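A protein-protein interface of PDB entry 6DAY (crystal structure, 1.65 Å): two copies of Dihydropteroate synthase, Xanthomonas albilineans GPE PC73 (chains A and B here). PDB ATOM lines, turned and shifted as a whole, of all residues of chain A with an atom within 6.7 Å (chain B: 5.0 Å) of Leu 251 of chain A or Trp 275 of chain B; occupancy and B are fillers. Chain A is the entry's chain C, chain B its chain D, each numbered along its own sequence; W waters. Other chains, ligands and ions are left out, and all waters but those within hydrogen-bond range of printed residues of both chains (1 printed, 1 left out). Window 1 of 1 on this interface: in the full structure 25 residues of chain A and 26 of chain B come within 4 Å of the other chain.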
ATOM      1  N   LEU A 206      16.557 -17.304  -9.771  1.00  0.00           N
ATOM      2  CA  LEU A 206      16.586 -18.182  -8.601  1.00  0.00           C
ATOM      3  C   LEU A 206      17.563 -17.645  -7.563  1.00  0.00           C
ATOM      4  O   LEU A 206      17.225 -17.518  -6.377  1.00  0.00           O
ATOM      5  CB  LEU A 206      16.925 -19.615  -9.042  1.00  0.00           C
ATOM      6  CG  LEU A 206      16.951 -20.695  -7.955  1.00  0.00           C
ATOM      7  CD1 LEU A 206      15.690 -20.718  -7.103  1.00  0.00           C
ATOM      8  CD2 LEU A 206      17.184 -22.089  -8.616  1.00  0.00           C
ATOM      9  N   LEU A 209      15.953 -14.600  -5.912  1.00  0.00           N
ATOM     10  CA  LEU A 209      14.563 -14.756  -5.531  1.00  0.00           C
ATOM     11  C   LEU A 209      14.202 -14.045  -4.229  1.00  0.00           C
ATOM     12  O   LEU A 209      13.045 -13.611  -4.117  1.00  0.00           O
ATOM     13  CB  LEU A 209      14.221 -16.252  -5.466  1.00  0.00           C
ATOM     14  CG  LEU A 209      12.747 -16.644  -5.516  1.00  0.00           C
ATOM     15  CD1 LEU A 209      12.052 -16.320  -6.856  1.00  0.00           C
ATOM     16  CD2 LEU A 209      12.655 -18.156  -5.292  1.00  0.00           C
ATOM     17  N   LEU A 232      21.595 -27.297 -17.028  1.00  0.00           N
ATOM     18  CA  LEU A 232      22.586 -27.237 -15.960  1.00  0.00           C
ATOM     19  C   LEU A 232      23.170 -28.611 -15.685  1.00  0.00           C
ATOM     20  O   LEU A 232      24.344 -28.728 -15.368  1.00  0.00           O
ATOM     21  CB  LEU A 232      21.970 -26.703 -14.659  1.00  0.00           C
ATOM     22  CG  LEU A 232      21.572 -25.211 -14.671  1.00  0.00           C
ATOM     23  CD1 LEU A 232      20.864 -24.884 -13.337  1.00  0.00           C
ATOM     24  CD2 LEU A 232      22.770 -24.331 -14.931  1.00  0.00           C
ATOM     25  N   VAL A 246      14.203 -31.296  -7.967  1.00  0.00           N
ATOM     26  CA  VAL A 246      13.987 -31.299  -6.529  1.00  0.00           C
ATOM     27  C   VAL A 246      14.986 -30.373  -5.854  1.00  0.00           C
ATOM     28  O   VAL A 246      14.632 -29.620  -4.943  1.00  0.00           O
ATOM     29  CB  VAL A 246      14.066 -32.733  -5.976  1.00  0.00           C
ATOM     30  CG1 VAL A 246      13.906 -32.663  -4.470  1.00  0.00           C
ATOM     31  CG2 VAL A 246      12.884 -33.547  -6.579  1.00  0.00           C
ATOM     32  N   ALA A 247      16.224 -30.358  -6.341  1.00  0.00           N
ATOM     33  CA  ALA A 247      17.246 -29.487  -5.754  1.00  0.00           C
ATOM     34  C   ALA A 247      16.890 -28.020  -5.969  1.00  0.00           C
ATOM     35  O   ALA A 247      16.948 -27.214  -5.031  1.00  0.00           O
ATOM     36  CB  ALA A 247      18.634 -29.783  -6.356  1.00  0.00           C
ATOM     37  N   ALA A 248      16.479 -27.675  -7.198  1.00  0.00           N
ATOM     38  CA  ALA A 248      16.069 -26.294  -7.502  1.00  0.00           C
ATOM     39  C   ALA A 248      14.920 -25.842  -6.610  1.00  0.00           C
ATOM     40  O   ALA A 248      14.906 -24.684  -6.147  1.00  0.00           O
ATOM     41  CB  ALA A 248      15.687 -26.150  -8.989  1.00  0.00           C
ATOM     42  N   HIS A 249      13.942 -26.717  -6.365  1.00  0.00           N
ATOM     43  CA  HIS A 249      12.813 -26.350  -5.528  1.00  0.00           C
ATOM     44  C   HIS A 249      13.196 -26.211  -4.077  1.00  0.00           C
ATOM     45  O   HIS A 249      12.681 -25.313  -3.399  1.00  0.00           O
ATOM     46  CB  HIS A 249      11.671 -27.334  -5.717  1.00  0.00           C
ATOM     47  CG  HIS A 249      10.997 -27.140  -7.041  1.00  0.00           C
ATOM     48  ND1 HIS A 249      10.822 -28.165  -7.951  1.00  0.00           N
ATOM     49  CD2 HIS A 249      10.507 -26.021  -7.634  1.00  0.00           C
ATOM     50  CE1 HIS A 249      10.251 -27.681  -9.047  1.00  0.00           C
ATOM     51  NE2 HIS A 249      10.032 -26.389  -8.871  1.00  0.00           N
ATOM     52  N   LEU A 250      14.147 -27.035  -3.581  1.00  0.00           N
ATOM     53  CA  LEU A 250      14.648 -26.815  -2.231  1.00  0.00           C
ATOM     54  C   LEU A 250      15.360 -25.471  -2.125  1.00  0.00           C
ATOM     55  O   LEU A 250      15.124 -24.701  -1.181  1.00  0.00           O
ATOM     56  CB  LEU A 250      15.574 -27.987  -1.849  1.00  0.00           C
ATOM     57  CG  LEU A 250      16.270 -27.781  -0.514  1.00  0.00           C
ATOM     58  CD1 LEU A 250      15.227 -27.565   0.563  1.00  0.00           C
ATOM     59  CD2 LEU A 250      17.130 -29.032  -0.164  1.00  0.00           C
ATOM     60  N   LEU A 251      16.170 -25.135  -3.131  1.00  0.00           N
ATOM     61  CA  LEU A 251      16.852 -23.852  -3.154  1.00  0.00           C
ATOM     62  C   LEU A 251      15.845 -22.710  -3.206  1.00  0.00           C
ATOM     63  O   LEU A 251      16.019 -21.718  -2.497  1.00  0.00           O
ATOM     64  CB  LEU A 251      17.804 -23.754  -4.356  1.00  0.00           C
ATOM     65  CG  LEU A 251      18.978 -24.771  -4.395  1.00  0.00           C
ATOM     66  CD1 LEU A 251      19.769 -24.556  -5.683  1.00  0.00           C
ATOM     67  CD2 LEU A 251      19.888 -24.563  -3.185  1.00  0.00           C
ATOM     68  N   ALA A 252      14.784 -22.864  -3.979  1.00  0.00           N
ATOM     69  CA  ALA A 252      13.785 -21.792  -4.047  1.00  0.00           C
ATOM     70  C   ALA A 252      13.099 -21.609  -2.701  1.00  0.00           C
ATOM     71  O   ALA A 252      12.884 -20.476  -2.241  1.00  0.00           O
ATOM     72  CB  ALA A 252      12.743 -22.137  -5.126  1.00  0.00           C
ATOM     73  N   ALA A 253      12.773 -22.723  -2.029  1.00  0.00           N
ATOM     74  CA  ALA A 253      12.160 -22.610  -0.717  1.00  0.00           C
ATOM     75  C   ALA A 253      13.117 -21.954   0.267  1.00  0.00           C
ATOM     76  O   ALA A 253      12.698 -21.122   1.087  1.00  0.00           O
ATOM     77  CB  ALA A 253      11.744 -23.977  -0.168  1.00  0.00           C
ATOM     78  N   GLN A 254      14.413 -22.300   0.190  1.00  0.00           N
ATOM     79  CA  GLN A 254      15.364 -21.665   1.088  1.00  0.00           C
ATOM     80  C   GLN A 254      15.450 -20.175   0.865  1.00  0.00           C
ATOM     81  O   GLN A 254      15.800 -19.421   1.802  1.00  0.00           O
ATOM     82  CB  GLN A 254      16.769 -22.263   0.917  1.00  0.00           C
ATOM     83  CG  GLN A 254      16.806 -23.701   1.357  1.00  0.00           C
ATOM     84  CD  GLN A 254      18.170 -24.342   1.079  1.00  0.00           C
ATOM     85  OE1 GLN A 254      18.831 -24.011   0.087  1.00  0.00           O
ATOM     86  NE2 GLN A 254      18.629 -25.214   2.000  1.00  0.00           N
ATOM     87  N   ARG A 255      15.184 -19.737  -0.359  1.00  0.00           N
ATOM     88  CA  ARG A 255      15.272 -18.331  -0.730  1.00  0.00           C
ATOM     89  C   ARG A 255      13.925 -17.614  -0.661  1.00  0.00           C
ATOM     90  O   ARG A 255      13.829 -16.477  -1.126  1.00  0.00           O
ATOM     91  CB  ARG A 255      15.885 -18.187  -2.130  1.00  0.00           C
ATOM     92  CG  ARG A 255      17.355 -18.491  -2.092  1.00  0.00           C
ATOM     93  CD  ARG A 255      18.095 -18.666  -3.423  1.00  0.00           C
ATOM     94  NE  ARG A 255      19.404 -19.274  -3.108  1.00  0.00           N
ATOM     95  CZ  ARG A 255      20.585 -18.656  -3.141  1.00  0.00           C
ATOM     96  NH1 ARG A 255      20.705 -17.381  -3.522  1.00  0.00           N
ATOM     97  NH2 ARG A 255      21.667 -19.339  -2.810  1.00  0.00           N
ATOM     98  N   GLY A 256      12.899 -18.240  -0.085  1.00  0.00           N
ATOM     99  CA  GLY A 256      11.666 -17.568   0.278  1.00  0.00           C
ATOM    100  C   GLY A 256      10.431 -18.037  -0.439  1.00  0.00           C
ATOM    101  O   GLY A 256       9.345 -17.577  -0.074  1.00  0.00           O
ATOM    102  N   ALA A 257      10.545 -18.894  -1.453  1.00  0.00           N
ATOM    103  CA  ALA A 257       9.357 -19.341  -2.177  1.00  0.00           C
ATOM    104  C   ALA A 257       8.443 -20.085  -1.208  1.00  0.00           C
ATOM    105  O   ALA A 257       8.906 -20.904  -0.397  1.00  0.00           O
ATOM    106  CB  ALA A 257       9.743 -20.233  -3.375  1.00  0.00           C
ATOM    107  N   PRO B  20      32.343 -29.269  -2.971  1.00  0.00           N
ATOM    108  CA  PRO B  20      32.032 -30.613  -2.439  1.00  0.00           C
ATOM    109  C   PRO B  20      32.240 -31.685  -3.491  1.00  0.00           C
ATOM    110  O   PRO B  20      31.856 -31.525  -4.641  1.00  0.00           O
ATOM    111  CB  PRO B  20      30.560 -30.512  -2.033  1.00  0.00           C
ATOM    112  CG  PRO B  20      30.318 -29.062  -1.844  1.00  0.00           C
ATOM    113  CD  PRO B  20      31.199 -28.347  -2.829  1.00  0.00           C
ATOM    114  N   LEU B 250      22.907 -32.196   0.222  1.00  0.00           N
ATOM    115  CA  LEU B 250      22.996 -30.808  -0.189  1.00  0.00           C
ATOM    116  C   LEU B 250      23.059 -29.893   1.016  1.00  0.00           C
ATOM    117  O   LEU B 250      23.800 -28.914   1.007  1.00  0.00           O
ATOM    118  CB  LEU B 250      21.773 -30.485  -1.060  1.00  0.00           C
ATOM    119  CG  LEU B 250      21.649 -29.046  -1.497  1.00  0.00           C
ATOM    120  CD1 LEU B 250      22.853 -28.589  -2.297  1.00  0.00           C
ATOM    121  CD2 LEU B 250      20.374 -28.861  -2.344  1.00  0.00           C
ATOM    122  N   ALA B 253      26.585 -30.028   2.404  1.00  0.00           N
ATOM    123  CA  ALA B 253      27.485 -29.231   1.591  1.00  0.00           C
ATOM    124  C   ALA B 253      27.276 -27.730   1.833  1.00  0.00           C
ATOM    125  O   ALA B 253      28.249 -26.970   1.901  1.00  0.00           O
ATOM    126  CB  ALA B 253      27.264 -29.526   0.111  1.00  0.00           C
ATOM    127  N   GLN B 254      26.018 -27.282   1.972  1.00  0.00           N
ATOM    128  CA  GLN B 254      25.795 -25.861   2.246  1.00  0.00           C
ATOM    129  C   GLN B 254      26.389 -25.433   3.590  1.00  0.00           C
ATOM    130  O   GLN B 254      26.680 -24.251   3.786  1.00  0.00           O
ATOM    131  CB  GLN B 254      24.294 -25.551   2.224  1.00  0.00           C
ATOM    132  CG  GLN B 254      23.675 -25.683   0.849  1.00  0.00           C
ATOM    133  CD  GLN B 254      22.185 -25.495   0.900  1.00  0.00           C
ATOM    134  OE1 GLN B 254      21.532 -25.888   1.871  1.00  0.00           O
ATOM    135  NE2 GLN B 254      21.637 -24.830  -0.125  1.00  0.00           N
ATOM    136  N   ALA B 271      22.119 -32.466  -7.905  1.00  0.00           N
ATOM    137  CA  ALA B 271      21.714 -31.478  -6.903  1.00  0.00           C
ATOM    138  C   ALA B 271      22.829 -30.493  -6.618  1.00  0.00           C
ATOM    139  O   ALA B 271      22.592 -29.271  -6.531  1.00  0.00           O
ATOM    140  CB  ALA B 271      21.268 -32.149  -5.597  1.00  0.00           C
ATOM    141  N   LEU B 272      24.069 -30.998  -6.475  1.00  0.00           N
ATOM    142  CA  LEU B 272      25.198 -30.123  -6.211  1.00  0.00           C
ATOM    143  C   LEU B 272      25.471 -29.206  -7.387  1.00  0.00           C
ATOM    144  O   LEU B 272      25.905 -28.064  -7.184  1.00  0.00           O
ATOM    145  CB  LEU B 272      26.454 -30.964  -5.920  1.00  0.00           C
ATOM    146  CG  LEU B 272      26.359 -31.673  -4.591  1.00  0.00           C
ATOM    147  CD1 LEU B 272      27.568 -32.673  -4.483  1.00  0.00           C
ATOM    148  CD2 LEU B 272      26.417 -30.712  -3.415  1.00  0.00           C
ATOM    149  N   THR B 273      25.234 -29.696  -8.607  1.00  0.00           N
ATOM    150  CA  THR B 273      25.457 -28.894  -9.800  1.00  0.00           C
ATOM    151  C   THR B 273      24.482 -27.711  -9.874  1.00  0.00           C
ATOM    152  O   THR B 273      24.886 -26.602 -10.250  1.00  0.00           O
ATOM    153  CB  THR B 273      25.339 -29.776 -11.046  1.00  0.00           C
ATOM    154  OG1 THR B 273      26.368 -30.779 -11.021  1.00  0.00           O
ATOM    155  CG2 THR B 273      25.502 -28.979 -12.299  1.00  0.00           C
ATOM    156  N   VAL B 274      23.209 -27.930  -9.534  1.00  0.00           N
ATOM    157  CA  VAL B 274      22.254 -26.818  -9.558  1.00  0.00           C
ATOM    158  C   VAL B 274      22.630 -25.813  -8.486  1.00  0.00           C
ATOM    159  O   VAL B 274      22.595 -24.588  -8.711  1.00  0.00           O
ATOM    160  CB  VAL B 274      20.800 -27.320  -9.370  1.00  0.00           C
ATOM    161  CG1 VAL B 274      19.847 -26.117  -9.288  1.00  0.00           C
ATOM    162  CG2 VAL B 274      20.368 -28.201 -10.543  1.00  0.00           C
ATOM    163  N   TRP B 275      22.991 -26.320  -7.295  1.00  0.00           N
ATOM    164  CA  TRP B 275      23.388 -25.427  -6.206  1.00  0.00           C
ATOM    165  C   TRP B 275      24.622 -24.626  -6.575  1.00  0.00           C
ATOM    166  O   TRP B 275      24.677 -23.409  -6.332  1.00  0.00           O
ATOM    167  CB  TRP B 275      23.627 -26.251  -4.940  1.00  0.00           C
ATOM    168  CG  TRP B 275      24.220 -25.491  -3.849  1.00  0.00           C
ATOM    169  CD1 TRP B 275      23.732 -24.358  -3.238  1.00  0.00           C
ATOM    170  CD2 TRP B 275      25.449 -25.796  -3.218  1.00  0.00           C
ATOM    171  NE1 TRP B 275      24.594 -23.973  -2.236  1.00  0.00           N
ATOM    172  CE2 TRP B 275      25.663 -24.831  -2.220  1.00  0.00           C
ATOM    173  CE3 TRP B 275      26.390 -26.801  -3.398  1.00  0.00           C
ATOM    174  CZ2 TRP B 275      26.794 -24.845  -1.386  1.00  0.00           C
ATOM    175  CZ3 TRP B 275      27.520 -26.818  -2.571  1.00  0.00           C
ATOM    176  CH2 TRP B 275      27.705 -25.851  -1.580  1.00  0.00           C
ATOM    177  N   GLN B 276      25.614 -25.279  -7.204  1.00  0.00           N
ATOM    178  CA  GLN B 276      26.823 -24.554  -7.584  1.00  0.00           C
ATOM    179  C   GLN B 276      26.513 -23.420  -8.555  1.00  0.00           C
ATOM    180  O   GLN B 276      27.109 -22.342  -8.455  1.00  0.00           O
ATOM    181  CB  GLN B 276      27.846 -25.513  -8.189  1.00  0.00           C
ATOM    182  CG  GLN B 276      28.559 -26.379  -7.136  1.00  0.00           C
ATOM    183  CD  GLN B 276      29.560 -25.583  -6.300  1.00  0.00           C
ATOM    184  OE1 GLN B 276      30.070 -24.550  -6.732  1.00  0.00           O
ATOM    185  NE2 GLN B 276      29.827 -26.054  -5.092  1.00  0.00           N
ATOM    186  N   ALA B 277      25.578 -23.643  -9.497  1.00  0.00           N
ATOM    187  CA  ALA B 277      25.219 -22.599 -10.458  1.00  0.00           C
ATOM    188  C   ALA B 277      24.580 -21.410  -9.755  1.00  0.00           C
ATOM    189  O   ALA B 277      24.900 -20.257 -10.059  1.00  0.00           O
ATOM    190  CB  ALA B 277      24.260 -23.150 -11.520  1.00  0.00           C
ATOM    191  N   VAL B 278      23.703 -21.681  -8.786  1.00  0.00           N
ATOM    192  CA  VAL B 278      23.069 -20.607  -8.026  1.00  0.00           C
ATOM    193  C   VAL B 278      24.094 -19.872  -7.165  1.00  0.00           C
ATOM    194  O   VAL B 278      24.084 -18.637  -7.085  1.00  0.00           O
ATOM    195  CB  VAL B 278      21.943 -21.181  -7.153  1.00  0.00           C
ATOM    196  CG1 VAL B 278      21.440 -20.088  -6.216  1.00  0.00           C
ATOM    197  CG2 VAL B 278      20.802 -21.693  -8.037  1.00  0.00           C
ATOM    198  N   GLN B 279      24.979 -20.617  -6.497  1.00  0.00           N
ATOM    199  CA  GLN B 279      25.983 -20.001  -5.636  1.00  0.00           C
ATOM    200  C   GLN B 279      26.966 -19.149  -6.422  1.00  0.00           C
ATOM    201  O   GLN B 279      27.555 -18.226  -5.865  1.00  0.00           O
ATOM    202  CB  GLN B 279      26.745 -21.090  -4.875  1.00  0.00           C
ATOM    203  CG  GLN B 279      25.941 -21.682  -3.773  1.00  0.00           C
ATOM    204  CD  GLN B 279      26.333 -21.132  -2.422  1.00  0.00           C
ATOM    205  OE1 GLN B 279      27.502 -21.188  -2.031  1.00  0.00           O
ATOM    206  NE2 GLN B 279      25.356 -20.591  -1.698  1.00  0.00           N
ATOM    207  N   ALA B 280      27.185 -19.472  -7.699  1.00  0.00           N
ATOM    208  CA  ALA B 280      28.127 -18.736  -8.528  1.00  0.00           C
ATOM    209  C   ALA B 280      27.599 -17.370  -8.964  1.00  0.00           C
ATOM    210  O   ALA B 280      28.337 -16.618  -9.608  1.00  0.00           O
ATOM    211  CB  ALA B 280      28.486 -19.564  -9.767  1.00  0.00           C
HETATM  212  O   HOH W   1      23.513 -16.912  -4.967  1.00  0.00           O
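Hydrophobic or aromatic side chains of chain A that line the printed part of chain B: Leu 206, Leu 232, Ala 247, Leu 250 and Leu 251.
Along chain A the printed residues that touch a printed residue of chain B span positions 206 to 255.
Hydrophobic or aromatic side chains of chain B that line the printed part of chain A: Leu 250, Ala 271, Val 274, Trp 275, Ala 277 and Val 278.
Among the printed residues, no Asp or Glu carboxylate lies within 4 Å of a Lys or Arg side-chain nitrogen of the other chain.
OE1 of Gln 254 of chain A sits at hydrogen-bond distance from NE2 of Gln 254 of chain B (2.9 Å).
Val 278 of chain B touches Leu 206 of chain A (CG2 to CD2, 3.7 Å).
Leu 232 of chain A touches Thr 273 of chain B (O to CG2, 3.3 Å).
Leu 232 of chain A touches Ala 277 of chain B (CD2 to CB, 3.9 Å).
Ala 271 of chain B touches Ala 247 of chain A (CA to CB, 3.6 Å).
Leu 250 of chain B touches Leu 250 of chain A.
Leu 251 of chain A touches Gln 254 of chain B.
CG1 of Val 274 of chain B touches CD1 of Leu 251 of chain A, 3.9 Å away.
Leu 251 of chain A touches Trp 275 of chain B (CD1 to CA, 3.8 Å).
Val 278 of chain B touches Leu 251 of chain A (CG2 to CD1, 3.8 Å).
Arg 255 of chain A touches Val 278 of chain B (NH2 to CG1, 3.5 Å).
Leu 250 of chain B touches its own counterpart, Leu 250 of chain A.
Gln 254 of chain B touches its own counterpart, Gln 254 of chain A.
3 positions are printed for both chains.
Of the 11 pairs that touch across the chains among the printed residues, 2 have their exchanged pair printed and touching as well.
Water W1 lies within hydrogen-bond range of O of Val 278 of chain B and NH1 of Arg 255 of chain A.
Of chain B, only Gln 254, Val 274, Trp 275 and Val 278 come within 4 Å of Leu 251 of chain A.
Trp 275 of chain B touches just one residue of chain A: Leu 251 (3.8 Å).
Printed residues of chain B within 4 Å of Ala 247 of chain A: Ala 271.
Printed residues of chain B within 4 Å of Leu 206 of chain A: Val 278 (3.7 Å).
Of the printed residues of chain A, Val 278 of chain B touches Leu 206 (3.7 Å), Leu 251 (3.8 Å) and Arg 255 (3.5 Å).
Gly 256 of chain A touches none of the printed residues of chain B.
Ala 248 of chain A touches none of the printed residues of chain B.
The nearest residue of chain B that does not touch Leu 251 of chain A is Leu 250 of chain B (4.4 Å).
The nearest residue of chain A that does not touch Trp 275 of chain B is Arg 255 of chain A (5.4 Å).
The nearest printed residue of chain B that does not touch Leu 250 of chain A is Gln 254 of chain B (5.8 Å).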
